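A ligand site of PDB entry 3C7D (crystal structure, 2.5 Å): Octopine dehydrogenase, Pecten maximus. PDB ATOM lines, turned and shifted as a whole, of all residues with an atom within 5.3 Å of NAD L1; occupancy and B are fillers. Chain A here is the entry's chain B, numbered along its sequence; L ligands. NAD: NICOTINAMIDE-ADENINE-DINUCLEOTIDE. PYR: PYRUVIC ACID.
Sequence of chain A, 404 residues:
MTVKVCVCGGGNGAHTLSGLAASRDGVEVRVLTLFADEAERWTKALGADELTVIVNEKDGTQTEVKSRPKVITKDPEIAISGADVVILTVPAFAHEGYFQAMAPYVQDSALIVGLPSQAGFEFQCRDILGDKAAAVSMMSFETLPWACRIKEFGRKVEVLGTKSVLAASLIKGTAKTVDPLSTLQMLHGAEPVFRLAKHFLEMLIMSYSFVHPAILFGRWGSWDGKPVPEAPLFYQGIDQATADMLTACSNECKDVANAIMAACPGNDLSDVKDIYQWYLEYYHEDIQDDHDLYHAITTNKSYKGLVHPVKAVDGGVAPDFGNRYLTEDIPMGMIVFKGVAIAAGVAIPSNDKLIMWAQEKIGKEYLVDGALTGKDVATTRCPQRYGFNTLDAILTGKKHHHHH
N of Gly 11 is in hydrogen-bond range of O3B of NAD L1.
ND2 of Asn 12 lies within hydrogen-bond range of O1N of NAD L1 (2.7 Å).
The guanidinium group of Arg 324 is in salt-bridge range of an oxygen (O1A) of NAD L1 (3.1 Å).
N of Gly 13 sits at hydrogen-bond distance from O2N of NAD L1 (3.0 Å).
An oxygen (O7N) of NAD L1 lies within hydrogen-bond range of the backbone NH of Cys 148 (2.8 Å).
The side-chain amide oxygen (OE1) of Gln 118 lies close to an oxygen (O) of PYR L2, 2.6 Å away.
The backbone carbonyl oxygen of Gly 10 lies close to an oxygen (O3B) of NAD L1 (3.4 Å).
O3B of NAD L1 sits at hydrogen-bond distance from OE2 of Glu 38 (2.7 Å).
An oxygen (O2B) of NAD L1 is in hydrogen-bond range of the backbone NH (N) of Gly 10, 3.3 Å away.
The backbone NH (N) of Asn 12 lies within hydrogen-bond range of an oxygen (O2A) of NAD L1 (3.1 Å).
A nitrogen (N7N) of NAD L1 lies within hydrogen-bond range of the backbone carbonyl oxygen (O) of Cys 148 (3.3 Å).
The side-chain hydroxyl (OG1) of Thr 143 sits at hydrogen-bond distance from an oxygen (O) of PYR L2 (2.8 Å).
OE2 of Glu 328 is in hydrogen-bond range of N of Ala 92, at 3.1 Å.
The side-chain carboxylate of Glu 38 lies within hydrogen-bond range of the side-chain hydroxyl of Thr 33, at 2.7 Å.
N of Phe 93 lies within hydrogen-bond range of OE2 of Glu 328.
The side-chain hydroxyl of Thr 33 lies close to the side-chain hydroxyl of Tyr 98 (3.4 Å).
Gly 9 touches NAD L1.
Thr 33 touches NAD L1 (OG1 to O2B, 3.7 Å).
Phe 35 touches NAD L1 (CE1 to N6A, 3.3 Å).
Val 90 touches NAD L1 (CG1 to O4B, 3.6 Å).
CD of Pro 91 touches O5B of NAD L1, at 3.6 Å.
CZ of Phe 93 touches N7A of NAD L1, at 3.3 Å.
Ala 94 touches NAD L1.
Pro 116 touches NAD L1.
OG1 of Thr 143 touches C6N of NAD L1, at 3.6 Å.
Leu 144 touches NAD L1 (CD2 to N7N, 3.6 Å).
Trp 146 touches NAD L1 (O to O7N, 3.6 Å).
CA of Ala 147 touches O7N of NAD L1 (3.3 Å).
Glu 328 touches NAD L1 (OE1 to O3D, 3.9 Å).
The nearest printed residue that does not touch NAD L1 is Tyr 98 (4.2 Å).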
ATOM      1  N   GLY A   9      -2.881 -16.427 -10.220  1.00  0.00           N
ATOM      2  CA  GLY A   9      -3.595 -15.898 -11.382  1.00  0.00           C
ATOM      3  C   GLY A   9      -3.672 -14.383 -11.363  1.00  0.00           C
ATOM      4  O   GLY A   9      -3.305 -13.747 -10.365  1.00  0.00           O
ATOM      5  N   GLY A  10      -4.162 -13.810 -12.449  1.00  0.00           N
ATOM      6  CA  GLY A  10      -4.281 -12.360 -12.589  1.00  0.00           C
ATOM      7  C   GLY A  10      -5.514 -11.909 -13.362  1.00  0.00           C
ATOM      8  O   GLY A  10      -5.667 -10.718 -13.645  1.00  0.00           O
ATOM      9  N   GLY A  11      -6.386 -12.856 -13.691  1.00  0.00           N
ATOM     10  CA  GLY A  11      -7.628 -12.578 -14.413  1.00  0.00           C
ATOM     11  C   GLY A  11      -8.754 -12.080 -13.528  1.00  0.00           C
ATOM     12  O   GLY A  11      -8.510 -11.530 -12.445  1.00  0.00           O
ATOM     13  N   ASN A  12      -9.993 -12.274 -13.984  1.00  0.00           N
ATOM     14  CA  ASN A  12     -11.175 -11.764 -13.285  1.00  0.00           C
ATOM     15  C   ASN A  12     -11.317 -12.317 -11.872  1.00  0.00           C
ATOM     16  O   ASN A  12     -11.437 -11.554 -10.911  1.00  0.00           O
ATOM     17  CB  ASN A  12     -12.460 -12.036 -14.079  1.00  0.00           C
ATOM     18  CG  ASN A  12     -12.377 -11.533 -15.519  1.00  0.00           C
ATOM     19  OD1 ASN A  12     -12.188 -10.341 -15.772  1.00  0.00           O
ATOM     20  ND2 ASN A  12     -12.535 -12.458 -16.459  1.00  0.00           N
ATOM     21  N   GLY A  13     -11.286 -13.645 -11.773  1.00  0.00           N
ATOM     22  CA  GLY A  13     -11.423 -14.338 -10.493  1.00  0.00           C
ATOM     23  C   GLY A  13     -10.339 -13.984  -9.489  1.00  0.00           C
ATOM     24  O   GLY A  13     -10.621 -13.770  -8.313  1.00  0.00           O
ATOM     25  N   ALA A  14      -9.098 -13.921  -9.971  1.00  0.00           N
ATOM     26  CA  ALA A  14      -7.943 -13.587  -9.132  1.00  0.00           C
ATOM     27  C   ALA A  14      -8.060 -12.204  -8.517  1.00  0.00           C
ATOM     28  O   ALA A  14      -7.673 -12.006  -7.360  1.00  0.00           O
ATOM     29  CB  ALA A  14      -6.665 -13.704  -9.936  1.00  0.00           C
ATOM     30  N   THR A  33       1.579 -14.638  -9.783  1.00  0.00           N
ATOM     31  CA  THR A  33       1.304 -14.778 -11.207  1.00  0.00           C
ATOM     32  C   THR A  33       2.583 -14.906 -12.037  1.00  0.00           C
ATOM     33  O   THR A  33       3.503 -14.093 -11.909  1.00  0.00           O
ATOM     34  CB  THR A  33       0.336 -13.683 -11.762  1.00  0.00           C
ATOM     35  OG1 THR A  33       0.229 -13.814 -13.190  1.00  0.00           O
ATOM     36  CG2 THR A  33       0.803 -12.296 -11.416  1.00  0.00           C
ATOM     37  N   LEU A  34       2.637 -15.941 -12.867  1.00  0.00           N
ATOM     38  CA  LEU A  34       3.829 -16.284 -13.630  1.00  0.00           C
ATOM     39  C   LEU A  34       3.691 -15.895 -15.100  1.00  0.00           C
ATOM     40  O   LEU A  34       4.601 -16.145 -15.909  1.00  0.00           O
ATOM     41  CB  LEU A  34       4.123 -17.786 -13.515  1.00  0.00           C
ATOM     42  CG  LEU A  34       4.064 -18.433 -12.127  1.00  0.00           C
ATOM     43  CD1 LEU A  34       3.830 -19.932 -12.259  1.00  0.00           C
ATOM     44  CD2 LEU A  34       5.324 -18.149 -11.309  1.00  0.00           C
ATOM     45  N   PHE A  35       2.558 -15.284 -15.452  1.00  0.00           N
ATOM     46  CA  PHE A  35       2.325 -14.833 -16.814  1.00  0.00           C
ATOM     47  C   PHE A  35       3.143 -13.572 -17.101  1.00  0.00           C
ATOM     48  O   PHE A  35       2.744 -12.458 -16.729  1.00  0.00           O
ATOM     49  CB  PHE A  35       0.831 -14.604 -17.070  1.00  0.00           C
ATOM     50  CG  PHE A  35       0.501 -14.208 -18.490  1.00  0.00           C
ATOM     51  CD1 PHE A  35       1.176 -14.778 -19.564  1.00  0.00           C
ATOM     52  CD2 PHE A  35      -0.519 -13.289 -18.747  1.00  0.00           C
ATOM     53  CE1 PHE A  35       0.870 -14.407 -20.878  1.00  0.00           C
ATOM     54  CE2 PHE A  35      -0.830 -12.926 -20.051  1.00  0.00           C
ATOM     55  CZ  PHE A  35      -0.134 -13.490 -21.119  1.00  0.00           C
ATOM     56  N   GLU A  38       3.069  -9.851 -15.244  1.00  0.00           N
ATOM     57  CA  GLU A  38       1.730  -9.411 -14.830  1.00  0.00           C
ATOM     58  C   GLU A  38       1.692  -8.913 -13.382  1.00  0.00           C
ATOM     59  O   GLU A  38       0.923  -8.007 -13.059  1.00  0.00           O
ATOM     60  CB  GLU A  38       0.725 -10.549 -15.013  1.00  0.00           C
ATOM     61  CG  GLU A  38      -0.746 -10.128 -14.966  1.00  0.00           C
ATOM     62  CD  GLU A  38      -1.679 -11.283 -15.247  1.00  0.00           C
ATOM     63  OE1 GLU A  38      -1.573 -12.332 -14.573  1.00  0.00           O
ATOM     64  OE2 GLU A  38      -2.543 -11.140 -16.149  1.00  0.00           O
ATOM     65  N   THR A  89      -6.847 -19.649  -9.345  1.00  0.00           N
ATOM     66  CA  THR A  89      -7.967 -19.075 -10.089  1.00  0.00           C
ATOM     67  C   THR A  89      -7.487 -18.573 -11.465  1.00  0.00           C
ATOM     68  O   THR A  89      -7.216 -17.383 -11.660  1.00  0.00           O
ATOM     69  CB  THR A  89      -8.678 -17.965  -9.305  1.00  0.00           C
ATOM     70  OG1 THR A  89      -9.033 -18.446  -8.002  1.00  0.00           O
ATOM     71  CG2 THR A  89      -9.934 -17.514 -10.025  1.00  0.00           C
ATOM     72  N   VAL A  90      -7.372 -19.523 -12.391  1.00  0.00           N
ATOM     73  CA  VAL A  90      -6.960 -19.277 -13.775  1.00  0.00           C
ATOM     74  C   VAL A  90      -7.549 -20.368 -14.662  1.00  0.00           C
ATOM     75  O   VAL A  90      -7.940 -21.423 -14.161  1.00  0.00           O
ATOM     76  CB  VAL A  90      -5.412 -19.299 -13.952  1.00  0.00           C
ATOM     77  CG1 VAL A  90      -4.830 -17.915 -13.794  1.00  0.00           C
ATOM     78  CG2 VAL A  90      -4.739 -20.314 -13.021  1.00  0.00           C
ATOM     79  N   PRO A  91      -7.643 -20.110 -15.989  1.00  0.00           N
ATOM     80  CA  PRO A  91      -7.977 -21.177 -16.929  1.00  0.00           C
ATOM     81  C   PRO A  91      -7.011 -22.348 -16.774  1.00  0.00           C
ATOM     82  O   PRO A  91      -5.801 -22.142 -16.602  1.00  0.00           O
ATOM     83  CB  PRO A  91      -7.807 -20.512 -18.297  1.00  0.00           C
ATOM     84  CG  PRO A  91      -8.053 -19.068 -18.038  1.00  0.00           C
ATOM     85  CD  PRO A  91      -7.487 -18.803 -16.671  1.00  0.00           C
ATOM     86  N   ALA A  92      -7.540 -23.569 -16.847  1.00  0.00           N
ATOM     87  CA  ALA A  92      -6.805 -24.785 -16.520  1.00  0.00           C
ATOM     88  C   ALA A  92      -5.483 -25.002 -17.271  1.00  0.00           C
ATOM     89  O   ALA A  92      -4.621 -25.723 -16.775  1.00  0.00           O
ATOM     90  CB  ALA A  92      -7.698 -26.006 -16.670  1.00  0.00           C
ATOM     91  N   PHE A  93      -5.326 -24.389 -18.439  1.00  0.00           N
ATOM     92  CA  PHE A  93      -4.080 -24.522 -19.214  1.00  0.00           C
ATOM     93  C   PHE A  93      -2.875 -23.938 -18.474  1.00  0.00           C
ATOM     94  O   PHE A  93      -1.741 -24.360 -18.697  1.00  0.00           O
ATOM     95  CB  PHE A  93      -4.215 -23.936 -20.638  1.00  0.00           C
ATOM     96  CG  PHE A  93      -4.152 -22.428 -20.694  1.00  0.00           C
ATOM     97  CD1 PHE A  93      -5.321 -21.672 -20.756  1.00  0.00           C
ATOM     98  CD2 PHE A  93      -2.923 -21.762 -20.713  1.00  0.00           C
ATOM     99  CE1 PHE A  93      -5.268 -20.273 -20.820  1.00  0.00           C
ATOM    100  CE2 PHE A  93      -2.870 -20.358 -20.763  1.00  0.00           C
ATOM    101  CZ  PHE A  93      -4.041 -19.617 -20.819  1.00  0.00           C
ATOM    102  N   ALA A  94      -3.125 -22.971 -17.592  1.00  0.00           N
ATOM    103  CA  ALA A  94      -2.070 -22.322 -16.833  1.00  0.00           C
ATOM    104  C   ALA A  94      -1.669 -23.111 -15.579  1.00  0.00           C
ATOM    105  O   ALA A  94      -0.629 -22.841 -14.972  1.00  0.00           O
ATOM    106  CB  ALA A  94      -2.476 -20.907 -16.468  1.00  0.00           C
ATOM    107  N   TYR A  98       1.845 -23.261 -12.432  1.00  0.00           N
ATOM    108  CA  TYR A  98       1.679 -22.900 -11.022  1.00  0.00           C
ATOM    109  C   TYR A  98       2.073 -24.010 -10.062  1.00  0.00           C
ATOM    110  O   TYR A  98       2.707 -23.741  -9.041  1.00  0.00           O
ATOM    111  CB  TYR A  98       0.277 -22.381 -10.760  1.00  0.00           C
ATOM    112  CG  TYR A  98       0.086 -20.972 -11.262  1.00  0.00           C
ATOM    113  CD1 TYR A  98       0.562 -19.882 -10.534  1.00  0.00           C
ATOM    114  CD2 TYR A  98      -0.541 -20.723 -12.485  1.00  0.00           C
ATOM    115  CE1 TYR A  98       0.403 -18.576 -10.990  1.00  0.00           C
ATOM    116  CE2 TYR A  98      -0.700 -19.423 -12.954  1.00  0.00           C
ATOM    117  CZ  TYR A  98      -0.226 -18.365 -12.212  1.00  0.00           C
ATOM    118  OH  TYR A  98      -0.386 -17.080 -12.674  1.00  0.00           O
ATOM    119  N   PRO A 116     -11.793 -22.347 -10.343  1.00  0.00           N
ATOM    120  CA  PRO A 116     -11.629 -23.768 -10.654  1.00  0.00           C
ATOM    121  C   PRO A 116     -10.167 -23.953 -11.081  1.00  0.00           C
ATOM    122  O   PRO A 116      -9.496 -22.940 -11.344  1.00  0.00           O
ATOM    123  CB  PRO A 116     -12.572 -23.981 -11.844  1.00  0.00           C
ATOM    124  CG  PRO A 116     -13.371 -22.723 -11.968  1.00  0.00           C
ATOM    125  CD  PRO A 116     -12.502 -21.657 -11.436  1.00  0.00           C
ATOM    126  N   GLN A 118     -11.266 -27.484 -12.160  1.00  0.00           N
ATOM    127  CA  GLN A 118     -12.196 -28.356 -12.856  1.00  0.00           C
ATOM    128  C   GLN A 118     -11.482 -29.529 -13.505  1.00  0.00           C
ATOM    129  O   GLN A 118     -10.673 -30.017 -12.920  1.00  0.00           O
ATOM    130  CB  GLN A 118     -12.987 -27.567 -13.911  1.00  0.00           C
ATOM    131  CG  GLN A 118     -13.933 -26.526 -13.338  1.00  0.00           C
ATOM    132  CD  GLN A 118     -14.672 -25.754 -14.407  1.00  0.00           C
ATOM    133  OE1 GLN A 118     -15.443 -24.851 -14.106  1.00  0.00           O
ATOM    134  NE2 GLN A 118     -14.430 -26.114 -15.667  1.00  0.00           N
ATOM    135  N   THR A 143     -17.109 -24.645 -10.088  1.00  0.00           N
ATOM    136  CA  THR A 143     -16.984 -23.482 -10.979  1.00  0.00           C
ATOM    137  C   THR A 143     -16.425 -22.275 -10.213  1.00  0.00           C
ATOM    138  O   THR A 143     -16.066 -22.397  -9.042  1.00  0.00           O
ATOM    139  CB  THR A 143     -18.335 -23.146 -11.677  1.00  0.00           C
ATOM    140  OG1 THR A 143     -18.126 -22.153 -12.684  1.00  0.00           O
ATOM    141  CG2 THR A 143     -19.383 -22.643 -10.675  1.00  0.00           C
ATOM    142  N   LEU A 144     -16.350 -21.126 -10.868  1.00  0.00           N
ATOM    143  CA  LEU A 144     -16.014 -19.881 -10.174  1.00  0.00           C
ATOM    144  C   LEU A 144     -17.194 -19.421  -9.314  1.00  0.00           C
ATOM    145  O   LEU A 144     -18.350 -19.470  -9.767  1.00  0.00           O
ATOM    146  CB  LEU A 144     -15.615 -18.790 -11.177  1.00  0.00           C
ATOM    147  CG  LEU A 144     -14.868 -17.561 -10.628  1.00  0.00           C
ATOM    148  CD1 LEU A 144     -13.449 -17.917 -10.227  1.00  0.00           C
ATOM    149  CD2 LEU A 144     -14.843 -16.431 -11.648  1.00  0.00           C
ATOM    150  N   TRP A 146     -18.217 -16.513  -8.605  1.00  0.00           N
ATOM    151  CA  TRP A 146     -18.909 -15.329  -9.101  1.00  0.00           C
ATOM    152  C   TRP A 146     -18.895 -15.184 -10.613  1.00  0.00           C
ATOM    153  O   TRP A 146     -17.966 -15.647 -11.282  1.00  0.00           O
ATOM    154  CB  TRP A 146     -18.294 -14.053  -8.501  1.00  0.00           C
ATOM    155  CG  TRP A 146     -17.654 -14.215  -7.146  1.00  0.00           C
ATOM    156  CD1 TRP A 146     -18.240 -14.044  -5.927  1.00  0.00           C
ATOM    157  CD2 TRP A 146     -16.282 -14.560  -6.891  1.00  0.00           C
ATOM    158  NE1 TRP A 146     -17.322 -14.269  -4.926  1.00  0.00           N
ATOM    159  CE2 TRP A 146     -16.113 -14.592  -5.490  1.00  0.00           C
ATOM    160  CE3 TRP A 146     -15.185 -14.859  -7.716  1.00  0.00           C
ATOM    161  CZ2 TRP A 146     -14.893 -14.895  -4.889  1.00  0.00           C
ATOM    162  CZ3 TRP A 146     -13.965 -15.162  -7.116  1.00  0.00           C
ATOM    163  CH2 TRP A 146     -13.828 -15.181  -5.721  1.00  0.00           C
ATOM    164  N   ALA A 147     -19.919 -14.543 -11.151  1.00  0.00           N
ATOM    165  CA  ALA A 147     -19.842 -13.950 -12.484  1.00  0.00           C
ATOM    166  C   ALA A 147     -19.182 -12.585 -12.282  1.00  0.00           C
ATOM    167  O   ALA A 147     -19.774 -11.691 -11.685  1.00  0.00           O
ATOM    168  CB  ALA A 147     -21.227 -13.814 -13.096  1.00  0.00           C
ATOM    169  N   CYS A 148     -17.941 -12.455 -12.755  1.00  0.00           N
ATOM    170  CA  CYS A 148     -17.143 -11.262 -12.512  1.00  0.00           C
ATOM    171  C   CYS A 148     -16.292 -10.816 -13.709  1.00  0.00           C
ATOM    172  O   CYS A 148     -15.909 -11.633 -14.550  1.00  0.00           O
ATOM    173  CB  CYS A 148     -16.258 -11.446 -11.276  1.00  0.00           C
ATOM    174  SG  CYS A 148     -15.021 -12.753 -11.427  1.00  0.00           S
ATOM    175  N   ARG A 149     -16.008  -9.516 -13.766  1.00  0.00           N
ATOM    176  CA  ARG A 149     -15.154  -8.961 -14.809  1.00  0.00           C
ATOM    177  C   ARG A 149     -14.350  -7.779 -14.284  1.00  0.00           C
ATOM    178  O   ARG A 149     -14.836  -6.997 -13.471  1.00  0.00           O
ATOM    179  CB  ARG A 149     -15.976  -8.551 -16.033  1.00  0.00           C
ATOM    180  CG  ARG A 149     -15.166  -8.402 -17.327  1.00  0.00           C
ATOM    181  CD  ARG A 149     -16.057  -8.263 -18.551  1.00  0.00           C
ATOM    182  NE  ARG A 149     -16.564  -6.902 -18.730  1.00  0.00           N
ATOM    183  CZ  ARG A 149     -17.513  -6.553 -19.594  1.00  0.00           C
ATOM    184  NH1 ARG A 149     -18.078  -7.464 -20.380  1.00  0.00           N
ATOM    185  NH2 ARG A 149     -17.910  -5.293 -19.678  1.00  0.00           N
ATOM    186  N   ARG A 324     -13.186 -21.131 -25.673  1.00  0.00           N
ATOM    187  CA  ARG A 324     -12.996 -21.908 -24.449  1.00  0.00           C
ATOM    188  C   ARG A 324     -14.011 -23.033 -24.238  1.00  0.00           C
ATOM    189  O   ARG A 324     -13.812 -23.895 -23.386  1.00  0.00           O
ATOM    190  CB  ARG A 324     -13.004 -20.997 -23.209  1.00  0.00           C
ATOM    191  CG  ARG A 324     -11.752 -20.171 -23.011  1.00  0.00           C
ATOM    192  CD  ARG A 324     -11.326 -20.228 -21.557  1.00  0.00           C
ATOM    193  NE  ARG A 324     -11.097 -18.911 -20.968  1.00  0.00           N
ATOM    194  CZ  ARG A 324     -12.004 -18.219 -20.304  1.00  0.00           C
ATOM    195  NH1 ARG A 324     -13.233 -18.705 -20.132  1.00  0.00           N
ATOM    196  NH2 ARG A 324     -11.698 -17.029 -19.804  1.00  0.00           N
ATOM    197  N   GLU A 328     -10.864 -25.505 -23.803  1.00  0.00           N
ATOM    198  CA  GLU A 328     -10.765 -25.869 -22.399  1.00  0.00           C
ATOM    199  C   GLU A 328     -11.533 -27.152 -22.093  1.00  0.00           C
ATOM    200  O   GLU A 328     -10.969 -28.114 -21.560  1.00  0.00           O
ATOM    201  CB  GLU A 328     -11.248 -24.730 -21.502  1.00  0.00           C
ATOM    202  CG  GLU A 328     -10.230 -23.632 -21.247  1.00  0.00           C
ATOM    203  CD  GLU A 328      -9.552 -23.756 -19.884  1.00  0.00           C
ATOM    204  OE1 GLU A 328     -10.251 -24.024 -18.888  1.00  0.00           O
ATOM    205  OE2 GLU A 328      -8.312 -23.580 -19.821  1.00  0.00           O
HETATM  206  PA  NAD L   1      -9.290 -15.045 -17.080  1.00  0.00           P
HETATM  207  O1A NAD L   1      -9.391 -15.318 -18.532  1.00  0.00           O
HETATM  208  O2A NAD L   1      -9.804 -13.699 -16.752  1.00  0.00           O
HETATM  209  O5B NAD L   1      -7.761 -15.173 -16.596  1.00  0.00           O
HETATM  210  C5B NAD L   1      -6.682 -14.796 -17.422  1.00  0.00           C
HETATM  211  C4B NAD L   1      -5.407 -15.067 -16.632  1.00  0.00           C
HETATM  212  O4B NAD L   1      -4.817 -16.300 -17.021  1.00  0.00           O
HETATM  213  C3B NAD L   1      -4.340 -14.015 -16.841  1.00  0.00           C
HETATM  214  O3B NAD L   1      -4.500 -12.953 -15.942  1.00  0.00           O
HETATM  215  C2B NAD L   1      -3.066 -14.788 -16.590  1.00  0.00           C
HETATM  216  O2B NAD L   1      -2.730 -14.736 -15.225  1.00  0.00           O
HETATM  217  C1B NAD L   1      -3.401 -16.215 -16.974  1.00  0.00           C
HETATM  218  N9A NAD L   1      -2.827 -16.508 -18.303  1.00  0.00           N
HETATM  219  C8A NAD L   1      -3.399 -16.211 -19.520  1.00  0.00           C
HETATM  220  N7A NAD L   1      -2.577 -16.635 -20.503  1.00  0.00           N
HETATM  221  C5A NAD L   1      -1.488 -17.197 -19.943  1.00  0.00           C
HETATM  222  C6A NAD L   1      -0.346 -17.788 -20.486  1.00  0.00           C
HETATM  223  N6A NAD L   1      -0.037 -17.502 -21.753  1.00  0.00           N
HETATM  224  N1A NAD L   1       0.637 -18.290 -19.648  1.00  0.00           N
HETATM  225  C2A NAD L   1       0.494 -18.212 -18.276  1.00  0.00           C
HETATM  226  N3A NAD L   1      -0.656 -17.631 -17.745  1.00  0.00           N
HETATM  227  C4A NAD L   1      -1.620 -17.133 -18.558  1.00  0.00           C
HETATM  228  O3  NAD L   1     -10.073 -16.202 -16.266  1.00  0.00           O
HETATM  229  PN  NAD L   1     -11.111 -15.914 -15.056  1.00  0.00           P
HETATM  230  O1N NAD L   1     -12.161 -14.989 -15.510  1.00  0.00           O
HETATM  231  O2N NAD L   1     -10.343 -15.582 -13.832  1.00  0.00           O
HETATM  232  O5D NAD L   1     -11.818 -17.344 -14.861  1.00  0.00           O
HETATM  233  C5D NAD L   1     -11.098 -18.511 -14.525  1.00  0.00           C
HETATM  234  C4D NAD L   1     -11.981 -19.737 -14.758  1.00  0.00           C
HETATM  235  O4D NAD L   1     -13.262 -19.539 -14.205  1.00  0.00           O
HETATM  236  C3D NAD L   1     -12.166 -20.019 -16.247  1.00  0.00           C
HETATM  237  O3D NAD L   1     -11.839 -21.374 -16.488  1.00  0.00           O
HETATM  238  C2D NAD L   1     -13.637 -19.773 -16.518  1.00  0.00           C
HETATM  239  O2D NAD L   1     -14.171 -20.750 -17.391  1.00  0.00           O
HETATM  240  C1D NAD L   1     -14.286 -19.850 -15.140  1.00  0.00           C
HETATM  241  N1N NAD L   1     -15.436 -18.946 -14.988  1.00  0.00           N
HETATM  242  C2N NAD L   1     -15.332 -17.602 -15.241  1.00  0.00           C
HETATM  243  C3N NAD L   1     -16.426 -16.752 -15.071  1.00  0.00           C
HETATM  244  C7N NAD L   1     -16.185 -15.289 -14.829  1.00  0.00           C
HETATM  245  O7N NAD L   1     -17.298 -14.461 -14.581  1.00  0.00           O
HETATM  246  N7N NAD L   1     -14.947 -14.804 -14.839  1.00  0.00           N
HETATM  247  C4N NAD L   1     -17.646 -17.291 -14.651  1.00  0.00           C
HETATM  248  C5N NAD L   1     -17.751 -18.651 -14.391  1.00  0.00           C
HETATM  249  C6N NAD L   1     -16.640 -19.470 -14.559  1.00  0.00           C
HETATM  250  C   PYR L   2     -18.491 -23.672 -15.874  1.00  0.00           C
HETATM  251  O   PYR L   2     -17.792 -23.949 -14.776  1.00  0.00           O
HETATM  252  OXT PYR L   2     -17.965 -22.703 -16.695  1.00  0.00           O
HETATM  253  CA  PYR L   2     -19.737 -24.327 -16.200  1.00  0.00           C
HETATM  254  O3  PYR L   2     -20.002 -24.538 -17.539  1.00  0.00           O
HETATM  255  CB  PYR L   2     -20.767 -24.737 -15.104  1.00  0.00           C
